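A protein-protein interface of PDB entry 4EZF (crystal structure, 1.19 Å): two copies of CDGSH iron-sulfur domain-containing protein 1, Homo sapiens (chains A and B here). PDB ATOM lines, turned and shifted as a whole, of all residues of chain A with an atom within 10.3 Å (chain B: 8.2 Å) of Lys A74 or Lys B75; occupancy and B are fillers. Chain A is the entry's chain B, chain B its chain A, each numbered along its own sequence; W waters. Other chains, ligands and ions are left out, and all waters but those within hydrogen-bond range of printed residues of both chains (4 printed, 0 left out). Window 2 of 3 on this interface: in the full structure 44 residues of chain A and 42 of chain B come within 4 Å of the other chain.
The backbone NH (N) of Met B30 is in hydrogen-bond range of the backbone carbonyl oxygen (O) of Lys A73, at 3.0 Å.
O of Lys B73 is in hydrogen-bond range of N of Met A30, at 2.8 Å.
The backbone NH of Lys B73 sits at hydrogen-bond distance from the backbone carbonyl oxygen of Phe A28, 3.0 Å away.
The backbone NH (N) of Phe B28 is in hydrogen-bond range of the backbone carbonyl oxygen (O) of Ile A71 (2.9 Å).
The side-chain sulfur (SD) of Met B30 sits close to the backbone carbonyl oxygen (O) of Asp A35 (3.7 Å).
NZ of Lys A74 sits close to NZ of Lys B75 (3.1 Å).
The backbone carbonyl oxygen (O) of Phe B28 is in hydrogen-bond range of the backbone NH (N) of Lys A73, at 3.0 Å.
N of Lys A74 sits at hydrogen-bond distance from O of Ala A36 (2.9 Å).
The side-chain carboxylate (OD1) of Asp A29 lies within hydrogen-bond range of the backbone NH (N) of Glu A31, 3.0 Å away.
The side-chain amino group (NZ) of Lys B74 is in hydrogen-bond range of the backbone carbonyl oxygen (O) of Asp B29, at 3.3 Å.
The backbone carbonyl oxygen (O) of Ile A72 sits at hydrogen-bond distance from the backbone NH (N) of Ala A38 (2.9 Å).
The backbone carbonyl oxygen (O) of Met B30 is in hydrogen-bond range of the backbone NH (N) of Lys B75, at 2.9 Å.
The backbone NH of Asp B32 sits at hydrogen-bond distance from the backbone carbonyl oxygen of Lys B75, 3.0 Å away.
Among the printed residues, pairs that only touch across the chains: Phe A28 with Ile B72 (3.5 Å), Asp A29 with Lys B73 (3.7 Å), Met A30 with Met B30 (3.7 Å), Met A30 with Ile B72 (3.7 Å), Met A30 with Lys B75 (3.7 Å), Glu A31 with Lys B75 (3.8 Å), Ala A36 with Met B30 (3.5 Å), Lys A37 with Met B30 (3.7 Å), Ile A72 with Phe B28 (3.4 Å), Ile A72 with Met B30 (3.5 Å), Lys A73 with Asp B29 (3.3 Å), Lys A74 with Met B30 (3.9 Å) and Lys A74 with Glu B31 (3.2 Å).
Of the printed residues of chain B, Lys A74 touches Met B30 (3.9 Å), Glu B31 (3.2 Å) and Lys B75 (3.1 Å).
Of the printed residues of chain A, Lys B75 touches Met A30, Glu A31 and Lys A74.
Asp B32 touches none of the printed residues of chain A.
Printed residues of chain B within 4 Å of Asp A35: Met B30 (3.7 Å).
Printed residues of chain B within 4 Å of Lys A37: Met B30 (3.7 Å).
Of the printed residues of chain A, Lys B73 touches Phe A28 (3.0 Å), Asp A29 (3.7 Å) and Met A30 (2.8 Å).
Printed residues of chain B within 4 Å of Phe A28: Ile B72 (3.5 Å) and Lys B73 (3.0 Å).
Glu B76 touches none of the printed residues of chain A.
Ala A38 touches none of the printed residues of chain B.
The nearest printed residue of chain B that does not touch Lys A74 is Asp B29 (5.2 Å).
Hydrophobic or aromatic side chains of chain A that line the printed part of chain B: Met A30 and Ile A72.
Of the 15 printed residues of chain B, 7 touch a printed residue of chain A.
Hydrophobic or aromatic side chains of chain B within 4 Å of the printed part of chain A: Phe B28, Met B30 and Ile B72.
Met A30 touches its own counterpart, Met B30.
Met A30 touches Lys B73, and with the chains exchanged Lys A73 touches Met B30.
Asp A35 touches Met B30, but with the chains exchanged Met A30 does not touch Asp B35 (8.7 Å).
Lys A74 touches Met B30, but with the chains exchanged Met A30 does not touch Lys B74 (4.2 Å).
13 positions are printed for both chains.
Of the 20 pairs that touch across the chains among the printed residues, 11 have their exchanged pair printed and touching as well.
Water W1 bridges OE1 of Glu A31 (2.6 Å) and O of Glu B76 (2.7 Å).
Water W3 lies within hydrogen-bond range of OE2 of Glu A31 and N of Glu B76.
Water W2 bridges O of Lys B74 (2.7 Å) and OD1 of Asp A29 (2.7 Å).
Water W4 lies within hydrogen-bond range of the side-chain carboxylate (OD1) of Asp B29 and the backbone carbonyl oxygen (O) of Lys A73.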
ATOM      1  N   PHE A  28     -19.900   5.187   5.413  1.00  0.00           N
ATOM      2  CA  PHE A  28     -19.545   4.453   4.224  1.00  0.00           C
ATOM      3  C   PHE A  28     -18.066   4.645   3.915  1.00  0.00           C
ATOM      4  O   PHE A  28     -17.487   5.714   4.136  1.00  0.00           O
ATOM      5  CB  PHE A  28     -20.350   4.953   3.014  1.00  0.00           C
ATOM      6  CG  PHE A  28     -21.839   4.787   3.161  1.00  0.00           C
ATOM      7  CD1 PHE A  28     -22.414   3.534   2.999  1.00  0.00           C
ATOM      8  CD2 PHE A  28     -22.658   5.848   3.483  1.00  0.00           C
ATOM      9  CE1 PHE A  28     -23.784   3.337   3.142  1.00  0.00           C
ATOM     10  CE2 PHE A  28     -24.031   5.667   3.617  1.00  0.00           C
ATOM     11  CZ  PHE A  28     -24.599   4.412   3.441  1.00  0.00           C
ATOM     12  N   ASP A  29     -17.470   3.614   3.346  1.00  0.00           N
ATOM     13  CA  ASP A  29     -16.078   3.661   2.911  1.00  0.00           C
ATOM     14  C   ASP A  29     -16.086   3.644   1.379  1.00  0.00           C
ATOM     15  O   ASP A  29     -16.599   2.697   0.778  1.00  0.00           O
ATOM     16  CB  ASP A  29     -15.337   2.438   3.471  1.00  0.00           C
ATOM     17  CG  ASP A  29     -13.845   2.472   3.180  1.00  0.00           C
ATOM     18  OD1 ASP A  29     -13.436   3.192   2.246  1.00  0.00           O
ATOM     19  OD2 ASP A  29     -13.080   1.782   3.886  1.00  0.00           O
ATOM     20  N   MET A  30     -15.578   4.702   0.748  1.00  0.00           N
ATOM     21  CA  MET A  30     -15.619   4.805  -0.706  1.00  0.00           C
ATOM     22  C   MET A  30     -14.844   3.692  -1.404  1.00  0.00           C
ATOM     23  O   MET A  30     -15.098   3.406  -2.570  1.00  0.00           O
ATOM     24  CB  MET A  30     -15.143   6.183  -1.153  1.00  0.00           C
ATOM     25  CG  MET A  30     -16.036   7.334  -0.694  1.00  0.00           C
ATOM     26  SD  MET A  30     -17.772   7.288  -1.156  1.00  0.00           S
ATOM     27  CE  MET A  30     -18.523   6.332   0.161  1.00  0.00           C
ATOM     28  N   GLU A  31     -13.914   3.059  -0.695  1.00  0.00           N
ATOM     29  CA  GLU A  31     -13.204   1.896  -1.220  1.00  0.00           C
ATOM     30  C   GLU A  31     -14.174   0.777  -1.613  1.00  0.00           C
ATOM     31  O   GLU A  31     -13.902   0.013  -2.538  1.00  0.00           O
ATOM     32  CB  GLU A  31     -12.206   1.374  -0.184  1.00  0.00           C
ATOM     33  CG  GLU A  31     -11.189   0.371  -0.739  1.00  0.00           C
ATOM     34  CD  GLU A  31     -10.006   1.066  -1.398  1.00  0.00           C
ATOM     35  OE1 GLU A  31     -10.212   1.784  -2.396  1.00  0.00           O
ATOM     36  OE2 GLU A  31      -8.866   0.915  -0.899  1.00  0.00           O
ATOM     37  N   ASP A  32     -15.313   0.711  -0.922  1.00  0.00           N
ATOM     38  CA  ASP A  32     -16.278  -0.385  -1.062  1.00  0.00           C
ATOM     39  C   ASP A  32     -17.186  -0.214  -2.266  1.00  0.00           C
ATOM     40  O   ASP A  32     -17.828  -1.173  -2.693  1.00  0.00           O
ATOM     41  CB  ASP A  32     -17.187  -0.462   0.171  1.00  0.00           C
ATOM     42  CG  ASP A  32     -16.451  -0.868   1.442  1.00  0.00           C
ATOM     43  OD1 ASP A  32     -15.373  -1.497   1.367  1.00  0.00           O
ATOM     44  OD2 ASP A  32     -16.977  -0.562   2.534  1.00  0.00           O
ATOM     45  N   LEU A  33     -17.256   1.005  -2.794  1.00  0.00           N
ATOM     46  CA  LEU A  33     -18.175   1.339  -3.884  1.00  0.00           C
ATOM     47  C   LEU A  33     -17.666   0.951  -5.268  1.00  0.00           C
ATOM     48  O   LEU A  33     -16.477   1.059  -5.561  1.00  0.00           O
ATOM     49  CB  LEU A  33     -18.476   2.843  -3.881  1.00  0.00           C
ATOM     50  CG  LEU A  33     -19.704   3.317  -3.108  1.00  0.00           C
ATOM     51  CD1 LEU A  33     -19.634   2.904  -1.636  1.00  0.00           C
ATOM     52  CD2 LEU A  33     -19.877   4.825  -3.257  1.00  0.00           C
ATOM     53  N   GLY A  34     -18.584   0.509  -6.119  1.00  0.00           N
ATOM     54  CA  GLY A  34     -18.269   0.243  -7.510  1.00  0.00           C
ATOM     55  C   GLY A  34     -18.591   1.440  -8.384  1.00  0.00           C
ATOM     56  O   GLY A  34     -18.016   1.595  -9.466  1.00  0.00           O
ATOM     57  N   ASP A  35     -19.505   2.289  -7.921  1.00  0.00           N
ATOM     58  CA  ASP A  35     -19.943   3.449  -8.700  1.00  0.00           C
ATOM     59  C   ASP A  35     -19.019   4.658  -8.569  1.00  0.00           C
ATOM     60  O   ASP A  35     -18.210   4.750  -7.639  1.00  0.00           O
ATOM     61  CB  ASP A  35     -21.366   3.860  -8.310  1.00  0.00           C
ATOM     62  CG  ASP A  35     -22.400   2.836  -8.713  1.00  0.00           C
ATOM     63  OD1 ASP A  35     -22.037   1.650  -8.876  1.00  0.00           O
ATOM     64  OD2 ASP A  35     -23.581   3.223  -8.868  1.00  0.00           O
ATOM     65  N   ALA A  36     -19.164   5.594  -9.501  1.00  0.00           N
ATOM     66  CA  ALA A  36     -18.332   6.793  -9.515  1.00  0.00           C
ATOM     67  C   ALA A  36     -18.978   7.972  -8.781  1.00  0.00           C
ATOM     68  O   ALA A  36     -18.364   9.019  -8.638  1.00  0.00           O
ATOM     69  CB  ALA A  36     -17.987   7.187 -10.946  1.00  0.00           C
ATOM     70  N   LYS A  37     -20.211   7.785  -8.309  1.00  0.00           N
ATOM     71  CA  LYS A  37     -20.994   8.862  -7.693  1.00  0.00           C
ATOM     72  C   LYS A  37     -22.032   8.307  -6.706  1.00  0.00           C
ATOM     73  O   LYS A  37     -22.644   7.264  -6.968  1.00  0.00           O
ATOM     74  CB  LYS A  37     -21.701   9.649  -8.799  1.00  0.00           C
ATOM     75  CG  LYS A  37     -22.504  10.865  -8.369  1.00  0.00           C
ATOM     76  CD  LYS A  37     -23.244  11.458  -9.579  1.00  0.00           C
ATOM     77  CE  LYS A  37     -23.902  12.795  -9.260  1.00  0.00           C
ATOM     78  NZ  LYS A  37     -24.899  13.207 -10.288  1.00  0.00           N
ATOM     79  N   ALA A  38     -22.233   9.011  -5.589  1.00  0.00           N
ATOM     80  CA  ALA A  38     -23.305   8.732  -4.631  1.00  0.00           C
ATOM     81  C   ALA A  38     -23.930  10.061  -4.226  1.00  0.00           C
ATOM     82  O   ALA A  38     -23.221  11.042  -4.034  1.00  0.00           O
ATOM     83  CB  ALA A  38     -22.777   7.989  -3.414  1.00  0.00           C
ATOM     84  N   VAL A  39     -25.255  10.087  -4.100  1.00  0.00           N
ATOM     85  CA  VAL A  39     -25.974  11.315  -3.772  1.00  0.00           C
ATOM     86  C   VAL A  39     -26.771  11.070  -2.487  1.00  0.00           C
ATOM     87  O   VAL A  39     -27.716  10.265  -2.465  1.00  0.00           O
ATOM     88  CB  VAL A  39     -26.917  11.770  -4.914  1.00  0.00           C
ATOM     89  CG1 VAL A  39     -27.500  13.123  -4.594  1.00  0.00           C
ATOM     90  CG2 VAL A  39     -26.159  11.862  -6.244  1.00  0.00           C
ATOM     91  N   ILE A  71     -23.155  15.231  -2.498  1.00  0.00           N
ATOM     92  CA  ILE A  71     -22.676  14.349  -3.531  1.00  0.00           C
ATOM     93  C   ILE A  71     -21.206  13.990  -3.325  1.00  0.00           C
ATOM     94  O   ILE A  71     -20.364  14.855  -3.054  1.00  0.00           O
ATOM     95  CB  ILE A  71     -22.844  15.049  -4.906  1.00  0.00           C
ATOM     96  CG1 ILE A  71     -24.316  15.386  -5.123  1.00  0.00           C
ATOM     97  CG2 ILE A  71     -22.254  14.199  -6.021  1.00  0.00           C
ATOM     98  CD1 ILE A  71     -24.533  16.355  -6.264  1.00  0.00           C
ATOM     99  N   ILE A  72     -20.914  12.700  -3.421  1.00  0.00           N
ATOM    100  CA  ILE A  72     -19.525  12.249  -3.453  1.00  0.00           C
ATOM    101  C   ILE A  72     -19.278  11.667  -4.824  1.00  0.00           C
ATOM    102  O   ILE A  72     -20.001  10.785  -5.244  1.00  0.00           O
ATOM    103  CB  ILE A  72     -19.226  11.197  -2.361  1.00  0.00           C
ATOM    104  CG1 ILE A  72     -19.517  11.777  -0.970  1.00  0.00           C
ATOM    105  CG2 ILE A  72     -17.789  10.709  -2.490  1.00  0.00           C
ATOM    106  CD1 ILE A  72     -18.615  12.910  -0.534  1.00  0.00           C
ATOM    107  N   LYS A  73     -18.285  12.177  -5.539  1.00  0.00           N
ATOM    108  CA  LYS A  73     -18.087  11.730  -6.911  1.00  0.00           C
ATOM    109  C   LYS A  73     -16.642  11.836  -7.360  1.00  0.00           C
ATOM    110  O   LYS A  73     -15.863  12.637  -6.835  1.00  0.00           O
ATOM    111  CB  LYS A  73     -18.978  12.530  -7.857  1.00  0.00           C
ATOM    112  CG  LYS A  73     -18.623  14.006  -7.918  1.00  0.00           C
ATOM    113  CD  LYS A  73     -19.560  14.793  -8.861  1.00  0.00           C
ATOM    114  CE  LYS A  73     -19.235  16.290  -8.945  1.00  0.00           C
ATOM    115  N   LYS A  74     -16.272  10.968  -8.293  1.00  0.00           N
ATOM    116  CA  LYS A  74     -15.013  11.110  -9.016  1.00  0.00           C
ATOM    117  C   LYS A  74     -15.170  12.191 -10.097  1.00  0.00           C
ATOM    118  O   LYS A  74     -16.285  12.510 -10.501  1.00  0.00           O
ATOM    119  CB  LYS A  74     -14.619   9.773  -9.657  1.00  0.00           C
ATOM    120  CG  LYS A  74     -14.378   8.635  -8.682  1.00  0.00           C
ATOM    121  CD  LYS A  74     -14.150   7.319  -9.416  1.00  0.00           C
ATOM    122  CE  LYS A  74     -13.980   6.166  -8.443  1.00  0.00           C
ATOM    123  NZ  LYS A  74     -13.679   4.892  -9.166  1.00  0.00           N
ATOM    124  N   LYS A  75     -14.057  12.735 -10.578  1.00  0.00           N
ATOM    125  CA  LYS A  75     -14.079  13.768 -11.622  1.00  0.00           C
ATOM    126  C   LYS A  75     -14.686  13.261 -12.925  1.00  0.00           C
ATOM    127  O   LYS A  75     -14.627  12.066 -13.221  1.00  0.00           O
ATOM    128  CB  LYS A  75     -12.662  14.275 -11.883  1.00  0.00           C
ATOM    129  N   PHE B  28     -18.170  16.693  -3.277  1.00  0.00           N
ATOM    130  CA  PHE B  28     -16.777  16.495  -2.930  1.00  0.00           C
ATOM    131  C   PHE B  28     -16.207  15.312  -3.666  1.00  0.00           C
ATOM    132  O   PHE B  28     -16.928  14.393  -4.092  1.00  0.00           O
ATOM    133  CB  PHE B  28     -16.659  16.278  -1.415  1.00  0.00           C
ATOM    134  CG  PHE B  28     -16.958  17.502  -0.612  1.00  0.00           C
ATOM    135  CD1 PHE B  28     -16.030  18.546  -0.546  1.00  0.00           C
ATOM    136  CD2 PHE B  28     -18.164  17.649   0.030  1.00  0.00           C
ATOM    137  CE1 PHE B  28     -16.291  19.663   0.198  1.00  0.00           C
ATOM    138  CE2 PHE B  28     -18.446  18.782   0.760  1.00  0.00           C
ATOM    139  CZ  PHE B  28     -17.507  19.803   0.833  1.00  0.00           C
ATOM    140  N   ASP B  29     -14.891  15.315  -3.796  1.00  0.00           N
ATOM    141  CA  ASP B  29     -14.202  14.181  -4.386  1.00  0.00           C
ATOM    142  C   ASP B  29     -14.365  12.899  -3.579  1.00  0.00           C
ATOM    143  O   ASP B  29     -14.343  12.911  -2.332  1.00  0.00           O
ATOM    144  CB  ASP B  29     -12.716  14.482  -4.519  1.00  0.00           C
ATOM    145  CG  ASP B  29     -12.443  15.523  -5.522  1.00  0.00           C
ATOM    146  OD1 ASP B  29     -12.551  15.199  -6.723  1.00  0.00           O
ATOM    147  OD2 ASP B  29     -12.108  16.656  -5.110  1.00  0.00           O
ATOM    148  N   MET B  30     -14.524  11.802  -4.318  1.00  0.00           N
ATOM    149  CA  MET B  30     -14.561  10.458  -3.770  1.00  0.00           C
ATOM    150  C   MET B  30     -13.191   9.984  -3.325  1.00  0.00           C
ATOM    151  O   MET B  30     -13.073   9.246  -2.351  1.00  0.00           O
ATOM    152  CB  MET B  30     -15.136   9.514  -4.815  1.00  0.00           C
ATOM    153  CG  MET B  30     -15.376   8.118  -4.286  1.00  0.00           C
ATOM    154  SD  MET B  30     -16.241   7.058  -5.451  1.00  0.00           S
ATOM    155  CE  MET B  30     -17.914   7.706  -5.415  1.00  0.00           C
ATOM    156  N   GLU B  31     -12.177  10.430  -4.065  1.00  0.00           N
ATOM    157  CA  GLU B  31     -10.766  10.184  -3.798  1.00  0.00           C
ATOM    158  C   GLU B  31     -10.269  11.128  -2.720  1.00  0.00           C
ATOM    159  O   GLU B  31     -10.880  12.175  -2.482  1.00  0.00           O
ATOM    160  CB  GLU B  31      -9.947  10.411  -5.076  1.00  0.00           C
ATOM    161  CG  GLU B  31     -10.252   9.413  -6.181  1.00  0.00           C
ATOM    162  CD  GLU B  31     -10.624  10.068  -7.488  1.00  0.00           C
ATOM    163  OE1 GLU B  31     -10.228  11.232  -7.707  1.00  0.00           O
ATOM    164  OE2 GLU B  31     -11.343   9.433  -8.282  1.00  0.00           O
ATOM    165  N   ASP B  32      -9.135  10.781  -2.112  1.00  0.00           N
ATOM    166  CA  ASP B  32      -8.557  11.576  -1.019  1.00  0.00           C
ATOM    167  C   ASP B  32      -7.774  12.802  -1.496  1.00  0.00           C
ATOM    168  O   ASP B  32      -6.615  13.005  -1.125  1.00  0.00           O
ATOM    169  CB  ASP B  32      -7.710  10.699  -0.084  1.00  0.00           C
ATOM    170  CG  ASP B  32      -6.463  10.121  -0.758  1.00  0.00           C
ATOM    171  OD1 ASP B  32      -6.459   9.891  -1.988  1.00  0.00           O
ATOM    172  OD2 ASP B  32      -5.465   9.905  -0.047  1.00  0.00           O
ATOM    173  N   LEU B  33      -8.413  13.623  -2.329  1.00  0.00           N
ATOM    174  CA  LEU B  33      -7.803  14.864  -2.831  1.00  0.00           C
ATOM    175  C   LEU B  33      -7.892  16.012  -1.829  1.00  0.00           C
ATOM    176  O   LEU B  33      -7.043  16.909  -1.826  1.00  0.00           O
ATOM    177  CB  LEU B  33      -8.469  15.289  -4.142  1.00  0.00           C
ATOM    178  CG  LEU B  33      -8.128  14.361  -5.306  1.00  0.00           C
ATOM    179  CD1 LEU B  33      -8.961  14.684  -6.523  1.00  0.00           C
ATOM    180  CD2 LEU B  33      -6.641  14.417  -5.634  1.00  0.00           C
ATOM    181  N   ASP B  35      -9.252  15.383   1.696  1.00  0.00           N
ATOM    182  CA  ASP B  35      -9.160  14.853   3.044  1.00  0.00           C
ATOM    183  C   ASP B  35      -9.146  13.334   2.960  1.00  0.00           C
ATOM    184  O   ASP B  35      -9.378  12.770   1.890  1.00  0.00           O
ATOM    185  CB  ASP B  35     -10.293  15.396   3.945  1.00  0.00           C
ATOM    186  CG  ASP B  35     -11.697  15.218   3.347  1.00  0.00           C
ATOM    187  OD1 ASP B  35     -11.995  14.125   2.830  1.00  0.00           O
ATOM    188  OD2 ASP B  35     -12.536  16.141   3.460  1.00  0.00           O
ATOM    189  N   ALA B  36      -8.833  12.680   4.072  1.00  0.00           N
ATOM    190  CA  ALA B  36      -8.874  11.216   4.158  1.00  0.00           C
ATOM    191  C   ALA B  36     -10.266  10.715   4.515  1.00  0.00           C
ATOM    192  O   ALA B  36     -10.690   9.622   4.141  1.00  0.00           O
ATOM    193  CB  ALA B  36      -7.890  10.741   5.199  1.00  0.00           C
ATOM    194  N   LYS B  37     -10.979  11.538   5.261  1.00  0.00           N
ATOM    195  CA  LYS B  37     -12.276  11.173   5.767  1.00  0.00           C
ATOM    196  C   LYS B  37     -12.967  12.474   6.131  1.00  0.00           C
ATOM    197  O   LYS B  37     -12.312  13.472   6.450  1.00  0.00           O
ATOM    198  CB  LYS B  37     -12.102  10.255   6.982  1.00  0.00           C
ATOM    199  CG  LYS B  37     -13.364   9.772   7.633  1.00  0.00           C
ATOM    200  CD  LYS B  37     -13.069   9.209   8.990  1.00  0.00           C
ATOM    201  CE  LYS B  37     -14.177   9.547   9.952  1.00  0.00           C
ATOM    202  N   ILE B  72     -17.877   9.658   5.689  1.00  0.00           N
ATOM    203  CA  ILE B  72     -17.365   9.168   4.429  1.00  0.00           C
ATOM    204  C   ILE B  72     -15.853   9.047   4.513  1.00  0.00           C
ATOM    205  O   ILE B  72     -15.142  10.039   4.651  1.00  0.00           O
ATOM    206  CB  ILE B  72     -17.700  10.139   3.263  1.00  0.00           C
ATOM    207  CG1 ILE B  72     -19.204  10.347   3.132  1.00  0.00           C
ATOM    208  CG2 ILE B  72     -17.156   9.619   1.943  1.00  0.00           C
ATOM    209  CD1 ILE B  72     -19.965   9.108   2.710  1.00  0.00           C
ATOM    210  N   LYS B  73     -15.379   7.831   4.411  1.00  0.00           N
ATOM    211  CA  LYS B  73     -13.958   7.568   4.287  1.00  0.00           C
ATOM    212  C   LYS B  73     -13.607   7.600   2.797  1.00  0.00           C
ATOM    213  O   LYS B  73     -14.162   6.826   2.005  1.00  0.00           O
ATOM    214  CB  LYS B  73     -13.657   6.209   4.904  1.00  0.00           C
ATOM    215  CG  LYS B  73     -13.898   6.159   6.406  1.00  0.00           C
ATOM    216  CD  LYS B  73     -14.338   4.780   6.859  1.00  0.00           C
ATOM    217  CE  LYS B  73     -15.818   4.521   6.639  1.00  0.00           C
ATOM    218  NZ  LYS B  73     -16.645   5.604   7.211  1.00  0.00           N
ATOM    219  N   LYS B  74     -12.703   8.493   2.406  1.00  0.00           N
ATOM    220  CA  LYS B  74     -12.368   8.675   0.990  1.00  0.00           C
ATOM    221  C   LYS B  74     -11.533   7.518   0.453  1.00  0.00           C
ATOM    222  O   LYS B  74     -10.845   6.828   1.205  1.00  0.00           O
ATOM    223  CB  LYS B  74     -11.639  10.013   0.792  1.00  0.00           C
ATOM    224  CG  LYS B  74     -12.398  11.223   1.328  1.00  0.00           C
ATOM    225  CD  LYS B  74     -13.749  11.397   0.615  1.00  0.00           C
ATOM    226  CE  LYS B  74     -14.550  12.560   1.177  1.00  0.00           C
ATOM    227  NZ  LYS B  74     -13.906  13.831   0.840  1.00  0.00           N
ATOM    228  N   LYS B  75     -11.617   7.300  -0.854  1.00  0.00           N
ATOM    229  CA  LYS B  75     -10.840   6.276  -1.529  1.00  0.00           C
ATOM    230  C   LYS B  75      -9.396   6.745  -1.606  1.00  0.00           C
ATOM    231  O   LYS B  75      -9.119   7.788  -2.185  1.00  0.00           O
ATOM    232  CB  LYS B  75     -11.396   6.077  -2.937  1.00  0.00           C
ATOM    233  CG  LYS B  75     -10.529   5.237  -3.857  1.00  0.00           C
ATOM    234  CD  LYS B  75     -11.223   5.045  -5.193  1.00  0.00           C
ATOM    235  CE  LYS B  75     -11.584   3.598  -5.457  1.00  0.00           C
ATOM    236  NZ  LYS B  75     -12.266   3.475  -6.769  1.00  0.00           N
ATOM    237  N   GLU B  76      -8.468   5.981  -1.040  1.00  0.00           N
ATOM    238  CA  GLU B  76      -7.073   6.373  -1.106  1.00  0.00           C
ATOM    239  C   GLU B  76      -6.473   6.057  -2.461  1.00  0.00           C
ATOM    240  O   GLU B  76      -6.576   4.938  -2.957  1.00  0.00           O
ATOM    241  CB  GLU B  76      -6.292   5.635  -0.048  1.00  0.00           C
ATOM    242  CG  GLU B  76      -6.445   6.178   1.337  1.00  0.00           C
ATOM    243  CD  GLU B  76      -5.312   5.709   2.208  1.00  0.00           C
ATOM    244  OE1 GLU B  76      -5.086   4.477   2.267  1.00  0.00           O
ATOM    245  OE2 GLU B  76      -4.621   6.581   2.784  1.00  0.00           O
ATOM    246  N   THR B  77      -5.829   7.049  -3.058  1.00  0.00           N
ATOM    247  CA  THR B  77      -5.087   6.827  -4.293  1.00  0.00           C
ATOM    248  C   THR B  77      -3.583   6.796  -4.004  1.00  0.00           C
ATOM    249  O   THR B  77      -3.142   7.122  -2.887  1.00  0.00           O
ATOM    250  CB  THR B  77      -5.399   7.911  -5.310  1.00  0.00           C
ATOM    251  OG1 THR B  77      -4.985   9.176  -4.774  1.00  0.00           O
ATOM    252  CG2 THR B  77      -6.900   7.927  -5.610  1.00  0.00           C
ATOM    253  OXT THR B  77      -2.795   6.406  -4.864  1.00  0.00           O
HETATM  254  O   HOH W   1      -8.204   2.883  -3.632  1.00  0.00           O
HETATM  255  O   HOH W   2     -10.916   4.278   2.118  1.00  0.00           O
HETATM  256  O   HOH W   3      -9.116   3.344   0.097  1.00  0.00           O
HETATM  257  O   HOH W   4     -15.054  15.106  -7.825  1.00  0.00           O
